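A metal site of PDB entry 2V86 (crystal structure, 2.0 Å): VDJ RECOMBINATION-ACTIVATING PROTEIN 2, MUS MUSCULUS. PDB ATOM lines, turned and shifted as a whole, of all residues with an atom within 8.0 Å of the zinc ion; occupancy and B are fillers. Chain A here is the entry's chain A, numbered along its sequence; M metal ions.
NE2 of His 50 is in hydrogen-bond range of O of Tyr 10. The backbone NH (N) of Asp 19 sits close to the side-chain sulfur (SG) of Cys 53 (3.4 Å). SG of Cys 14 lies close to SG of Cys 15 (3.8 Å). The side-chain sulfur of Cys 18 sits close to the backbone NH of Val 20 (3.7 Å). The backbone carbonyl oxygen of Ile 12 lies close to the side-chain sulfur of Cys 18 (3.7 Å). The backbone NH of Cys 18 lies within hydrogen-bond range of the side-chain sulfur of Cys 15 (3.5 Å).
The zinc ion is bound by a ring nitrogen (ND1) of His 50, the side-chain sulfur (SG) of Cys 53, the side-chain sulfur (SG) of Cys 14 and the side-chain sulfur (SG) of Cys 18.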
ATOM      1  N   TYR A  10      -0.885 -18.883  35.665  1.00  0.00           N
ATOM      2  CA  TYR A  10      -0.258 -19.235  34.401  1.00  0.00           C
ATOM      3  C   TYR A  10      -1.152 -18.957  33.190  1.00  0.00           C
ATOM      4  O   TYR A  10      -0.664 -18.583  32.139  1.00  0.00           O
ATOM      5  CB  TYR A  10       0.098 -20.730  34.376  1.00  0.00           C
ATOM      6  CG  TYR A  10       1.395 -21.073  35.050  1.00  0.00           C
ATOM      7  CD1 TYR A  10       1.418 -21.555  36.358  1.00  0.00           C
ATOM      8  CD2 TYR A  10       2.602 -20.921  34.379  1.00  0.00           C
ATOM      9  CE1 TYR A  10       2.623 -21.882  36.980  1.00  0.00           C
ATOM     10  CE2 TYR A  10       3.805 -21.247  34.992  1.00  0.00           C
ATOM     11  CZ  TYR A  10       3.812 -21.722  36.283  1.00  0.00           C
ATOM     12  OH  TYR A  10       5.006 -22.068  36.866  1.00  0.00           O
ATOM     13  N   TRP A  11      -2.457 -19.122  33.368  1.00  0.00           N
ATOM     14  CA  TRP A  11      -3.371 -18.949  32.248  1.00  0.00           C
ATOM     15  C   TRP A  11      -4.135 -17.636  32.152  1.00  0.00           C
ATOM     16  O   TRP A  11      -5.281 -17.608  31.767  1.00  0.00           O
ATOM     17  CB  TRP A  11      -4.326 -20.139  32.214  1.00  0.00           C
ATOM     18  CG  TRP A  11      -3.567 -21.435  32.250  1.00  0.00           C
ATOM     19  CD1 TRP A  11      -3.418 -22.280  33.317  1.00  0.00           C
ATOM     20  CD2 TRP A  11      -2.773 -21.988  31.186  1.00  0.00           C
ATOM     21  NE1 TRP A  11      -2.588 -23.311  32.995  1.00  0.00           N
ATOM     22  CE2 TRP A  11      -2.178 -23.168  31.692  1.00  0.00           C
ATOM     23  CE3 TRP A  11      -2.512 -21.606  29.865  1.00  0.00           C
ATOM     24  CZ2 TRP A  11      -1.325 -23.962  30.918  1.00  0.00           C
ATOM     25  CZ3 TRP A  11      -1.671 -22.394  29.094  1.00  0.00           C
ATOM     26  CH2 TRP A  11      -1.085 -23.569  29.623  1.00  0.00           C
ATOM     27  N   ILE A  12      -3.466 -16.545  32.495  1.00  0.00           N
ATOM     28  CA  ILE A  12      -4.058 -15.217  32.426  1.00  0.00           C
ATOM     29  C   ILE A  12      -3.788 -14.663  31.031  1.00  0.00           C
ATOM     30  O   ILE A  12      -3.028 -15.235  30.269  1.00  0.00           O
ATOM     31  CB  ILE A  12      -3.392 -14.232  33.408  1.00  0.00           C
ATOM     32  CG1 ILE A  12      -1.885 -14.171  33.110  1.00  0.00           C
ATOM     33  CG2 ILE A  12      -3.650 -14.649  34.849  1.00  0.00           C
ATOM     34  CD1 ILE A  12      -1.145 -13.045  33.788  1.00  0.00           C
ATOM     35  N   THR A  13      -4.450 -13.562  30.708  1.00  0.00           N
ATOM     36  CA  THR A  13      -4.204 -12.883  29.438  1.00  0.00           C
ATOM     37  C   THR A  13      -3.188 -11.850  29.951  1.00  0.00           C
ATOM     38  O   THR A  13      -3.552 -10.801  30.423  1.00  0.00           O
ATOM     39  CB  THR A  13      -5.479 -12.178  28.923  1.00  0.00           C
ATOM     40  OG1 THR A  13      -6.484 -13.160  28.636  1.00  0.00           O
ATOM     41  CG2 THR A  13      -5.182 -11.374  27.659  1.00  0.00           C
ATOM     42  N   CYS A  14      -1.911 -12.221  29.871  1.00  0.00           N
ATOM     43  CA  CYS A  14      -0.819 -11.387  30.388  1.00  0.00           C
ATOM     44  C   CYS A  14      -0.654  -9.990  29.798  1.00  0.00           C
ATOM     45  O   CYS A  14      -0.071  -9.128  30.432  1.00  0.00           O
ATOM     46  CB  CYS A  14       0.508 -12.140  30.265  1.00  0.00           C
ATOM     47  SG  CYS A  14       1.223 -12.142  28.614  1.00  0.00           S
ATOM     48  N   CYS A  15      -1.154  -9.776  28.594  1.00  0.00           N
ATOM     49  CA  CYS A  15      -1.042  -8.466  27.950  1.00  0.00           C
ATOM     50  C   CYS A  15      -2.042  -8.394  26.800  1.00  0.00           C
ATOM     51  O   CYS A  15      -2.583  -9.400  26.395  1.00  0.00           O
ATOM     52  CB  CYS A  15       0.376  -8.258  27.423  1.00  0.00           C
ATOM     53  SG  CYS A  15       0.829  -9.357  26.092  1.00  0.00           S
ATOM     54  N   PRO A  16      -2.297  -7.177  26.277  1.00  0.00           N
ATOM     55  CA  PRO A  16      -3.243  -6.995  25.174  1.00  0.00           C
ATOM     56  C   PRO A  16      -3.069  -7.946  23.990  1.00  0.00           C
ATOM     57  O   PRO A  16      -4.033  -8.322  23.350  1.00  0.00           O
ATOM     58  CB  PRO A  16      -3.034  -5.534  24.784  1.00  0.00           C
ATOM     59  CG  PRO A  16      -2.665  -4.898  26.083  1.00  0.00           C
ATOM     60  CD  PRO A  16      -1.680  -5.896  26.662  1.00  0.00           C
ATOM     61  N   THR A  17      -1.830  -8.346  23.712  1.00  0.00           N
ATOM     62  CA  THR A  17      -1.576  -9.244  22.596  1.00  0.00           C
ATOM     63  C   THR A  17      -1.259 -10.665  23.044  1.00  0.00           C
ATOM     64  O   THR A  17      -0.694 -11.436  22.290  1.00  0.00           O
ATOM     65  CB  THR A  17      -0.429  -8.722  21.714  1.00  0.00           C
ATOM     66  OG1 THR A  17       0.774  -8.653  22.492  1.00  0.00           O
ATOM     67  CG2 THR A  17      -0.759  -7.346  21.164  1.00  0.00           C
ATOM     68  N   CYS A  18      -1.629 -11.009  24.267  1.00  0.00           N
ATOM     69  CA  CYS A  18      -1.378 -12.348  24.814  1.00  0.00           C
ATOM     70  C   CYS A  18      -1.840 -13.434  23.846  1.00  0.00           C
ATOM     71  O   CYS A  18      -3.001 -13.477  23.470  1.00  0.00           O
ATOM     72  CB  CYS A  18      -2.082 -12.526  26.156  1.00  0.00           C
ATOM     73  SG  CYS A  18      -1.734 -14.119  26.946  1.00  0.00           S
ATOM     74  N   ASP A  19      -0.918 -14.308  23.463  1.00  0.00           N
ATOM     75  CA  ASP A  19      -1.173 -15.387  22.514  1.00  0.00           C
ATOM     76  C   ASP A  19      -1.320 -16.757  23.193  1.00  0.00           C
ATOM     77  O   ASP A  19      -1.665 -17.728  22.566  1.00  0.00           O
ATOM     78  CB  ASP A  19      -0.011 -15.476  21.512  1.00  0.00           C
ATOM     79  CG  ASP A  19      -0.490 -15.653  20.088  1.00  0.00           C
ATOM     80  OD1 ASP A  19       0.216 -16.327  19.300  1.00  0.00           O
ATOM     81  OD2 ASP A  19      -1.550 -15.110  19.754  1.00  0.00           O
ATOM     82  N   VAL A  20      -1.030 -16.801  24.491  1.00  0.00           N
ATOM     83  CA  VAL A  20      -1.115 -18.041  25.247  1.00  0.00           C
ATOM     84  C   VAL A  20      -2.532 -18.355  25.685  1.00  0.00           C
ATOM     85  O   VAL A  20      -3.193 -17.538  26.308  1.00  0.00           O
ATOM     86  CB  VAL A  20      -0.184 -17.977  26.479  1.00  0.00           C
ATOM     87  CG1 VAL A  20      -0.325 -19.227  27.318  1.00  0.00           C
ATOM     88  CG2 VAL A  20       1.247 -17.795  26.020  1.00  0.00           C
ATOM     89  N   ASP A  21      -2.989 -19.567  25.364  1.00  0.00           N
ATOM     90  CA  ASP A  21      -4.336 -19.963  25.722  1.00  0.00           C
ATOM     91  C   ASP A  21      -4.400 -21.392  26.258  1.00  0.00           C
ATOM     92  O   ASP A  21      -3.898 -22.308  25.632  1.00  0.00           O
ATOM     93  CB  ASP A  21      -5.253 -19.830  24.497  1.00  0.00           C
ATOM     94  CG  ASP A  21      -6.688 -20.219  24.803  1.00  0.00           C
ATOM     95  OD1 ASP A  21      -7.537 -20.051  23.903  1.00  0.00           O
ATOM     96  OD2 ASP A  21      -6.988 -20.685  25.922  1.00  0.00           O
ATOM     97  N   PRO A  36       3.365 -22.560  30.397  1.00  0.00           N
ATOM     98  CA  PRO A  36       4.151 -21.530  29.720  1.00  0.00           C
ATOM     99  C   PRO A  36       5.168 -20.825  30.613  1.00  0.00           C
ATOM    100  O   PRO A  36       4.879 -20.532  31.763  1.00  0.00           O
ATOM    101  CB  PRO A  36       3.083 -20.570  29.197  1.00  0.00           C
ATOM    102  CG  PRO A  36       2.046 -20.629  30.277  1.00  0.00           C
ATOM    103  CD  PRO A  36       1.962 -22.120  30.578  1.00  0.00           C
ATOM    104  N   ALA A  37       6.352 -20.580  30.065  1.00  0.00           N
ATOM    105  CA  ALA A  37       7.394 -19.892  30.829  1.00  0.00           C
ATOM    106  C   ALA A  37       6.934 -18.450  31.067  1.00  0.00           C
ATOM    107  O   ALA A  37       6.326 -17.838  30.205  1.00  0.00           O
ATOM    108  CB  ALA A  37       8.709 -19.902  30.056  1.00  0.00           C
ATOM    109  N   MET A  38       7.229 -17.933  32.252  1.00  0.00           N
ATOM    110  CA  MET A  38       6.828 -16.568  32.586  1.00  0.00           C
ATOM    111  C   MET A  38       7.971 -15.747  33.173  1.00  0.00           C
ATOM    112  O   MET A  38       8.944 -16.290  33.678  1.00  0.00           O
ATOM    113  CB  MET A  38       5.637 -16.592  33.547  1.00  0.00           C
ATOM    114  CG  MET A  38       4.389 -17.234  32.940  1.00  0.00           C
ATOM    115  SD  MET A  38       2.924 -17.076  33.967  1.00  0.00           S
ATOM    116  CE  MET A  38       2.412 -15.417  33.543  1.00  0.00           C
ATOM    117  N   TRP A  48       3.161 -10.814  36.286  1.00  0.00           N
ATOM    118  CA  TRP A  48       3.836 -11.816  35.477  1.00  0.00           C
ATOM    119  C   TRP A  48       3.350 -11.812  34.033  1.00  0.00           C
ATOM    120  O   TRP A  48       2.176 -11.618  33.775  1.00  0.00           O
ATOM    121  CB  TRP A  48       3.598 -13.218  36.070  1.00  0.00           C
ATOM    122  CG  TRP A  48       4.235 -13.443  37.409  1.00  0.00           C
ATOM    123  CD1 TRP A  48       3.741 -13.092  38.625  1.00  0.00           C
ATOM    124  CD2 TRP A  48       5.506 -14.071  37.653  1.00  0.00           C
ATOM    125  NE1 TRP A  48       4.620 -13.465  39.619  1.00  0.00           N
ATOM    126  CE2 TRP A  48       5.716 -14.059  39.042  1.00  0.00           C
ATOM    127  CE3 TRP A  48       6.488 -14.631  36.826  1.00  0.00           C
ATOM    128  CZ2 TRP A  48       6.864 -14.594  39.634  1.00  0.00           C
ATOM    129  CZ3 TRP A  48       7.634 -15.165  37.407  1.00  0.00           C
ATOM    130  CH2 TRP A  48       7.809 -15.145  38.804  1.00  0.00           C
ATOM    131  N   VAL A  49       4.281 -12.002  33.104  1.00  0.00           N
ATOM    132  CA  VAL A  49       3.918 -12.054  31.683  1.00  0.00           C
ATOM    133  C   VAL A  49       4.499 -13.317  31.062  1.00  0.00           C
ATOM    134  O   VAL A  49       5.471 -13.846  31.537  1.00  0.00           O
ATOM    135  CB  VAL A  49       4.446 -10.824  30.897  1.00  0.00           C
ATOM    136  CG1 VAL A  49       3.712  -9.568  31.323  1.00  0.00           C
ATOM    137  CG2 VAL A  49       5.948 -10.671  31.116  1.00  0.00           C
ATOM    138  N   HIS A  50       3.848 -13.806  30.003  1.00  0.00           N
ATOM    139  CA  HIS A  50       4.320 -14.991  29.307  1.00  0.00           C
ATOM    140  C   HIS A  50       5.537 -14.601  28.474  1.00  0.00           C
ATOM    141  O   HIS A  50       5.494 -13.652  27.718  1.00  0.00           O
ATOM    142  CB  HIS A  50       3.238 -15.512  28.376  1.00  0.00           C
ATOM    143  CG  HIS A  50       2.011 -15.996  29.083  1.00  0.00           C
ATOM    144  ND1 HIS A  50       0.747 -15.561  28.775  1.00  0.00           N
ATOM    145  CD2 HIS A  50       1.869 -16.913  30.073  1.00  0.00           C
ATOM    146  CE1 HIS A  50      -0.134 -16.186  29.536  1.00  0.00           C
ATOM    147  NE2 HIS A  50       0.522 -17.008  30.336  1.00  0.00           N
ATOM    148  N   ALA A  51       6.631 -15.345  28.636  1.00  0.00           N
ATOM    149  CA  ALA A  51       7.860 -15.058  27.887  1.00  0.00           C
ATOM    150  C   ALA A  51       7.584 -15.004  26.392  1.00  0.00           C
ATOM    151  O   ALA A  51       8.051 -14.117  25.691  1.00  0.00           O
ATOM    152  CB  ALA A  51       8.902 -16.116  28.184  1.00  0.00           C
ATOM    153  N   GLN A  52       6.811 -15.976  25.914  1.00  0.00           N
ATOM    154  CA  GLN A  52       6.457 -16.101  24.508  1.00  0.00           C
ATOM    155  C   GLN A  52       5.747 -14.853  23.988  1.00  0.00           C
ATOM    156  O   GLN A  52       5.987 -14.391  22.891  1.00  0.00           O
ATOM    157  CB  GLN A  52       5.553 -17.320  24.339  1.00  0.00           C
ATOM    158  CG  GLN A  52       5.513 -17.915  22.964  1.00  0.00           C
ATOM    159  CD  GLN A  52       4.631 -19.154  22.933  1.00  0.00           C
ATOM    160  OE1 GLN A  52       3.412 -19.064  22.863  1.00  0.00           O
ATOM    161  NE2 GLN A  52       5.250 -20.322  23.005  1.00  0.00           N
ATOM    162  N   CYS A  53       4.856 -14.304  24.817  1.00  0.00           N
ATOM    163  CA  CYS A  53       4.092 -13.127  24.448  1.00  0.00           C
ATOM    164  C   CYS A  53       4.953 -11.868  24.351  1.00  0.00           C
ATOM    165  O   CYS A  53       4.582 -10.912  23.715  1.00  0.00           O
ATOM    166  CB  CYS A  53       2.959 -12.911  25.451  1.00  0.00           C
ATOM    167  SG  CYS A  53       1.787 -14.295  25.492  1.00  0.00           S
ATOM    168  N   MET A  54       6.114 -11.893  25.000  1.00  0.00           N
ATOM    169  CA  MET A  54       7.022 -10.754  24.968  1.00  0.00           C
ATOM    170  C   MET A  54       7.937 -10.847  23.741  1.00  0.00           C
ATOM    171  O   MET A  54       8.797 -10.012  23.529  1.00  0.00           O
ATOM    172  CB  MET A  54       7.857 -10.698  26.251  1.00  0.00           C
ATOM    173  CG  MET A  54       7.056 -10.508  27.532  1.00  0.00           C
ATOM    174  SD  MET A  54       6.107  -8.949  27.591  1.00  0.00           S
ATOM    175  CE  MET A  54       4.437  -9.545  27.197  1.00  0.00           C
HETATM  176 ZN    ZN M   1       0.575 -14.038  27.445  1.00  0.00          ZN
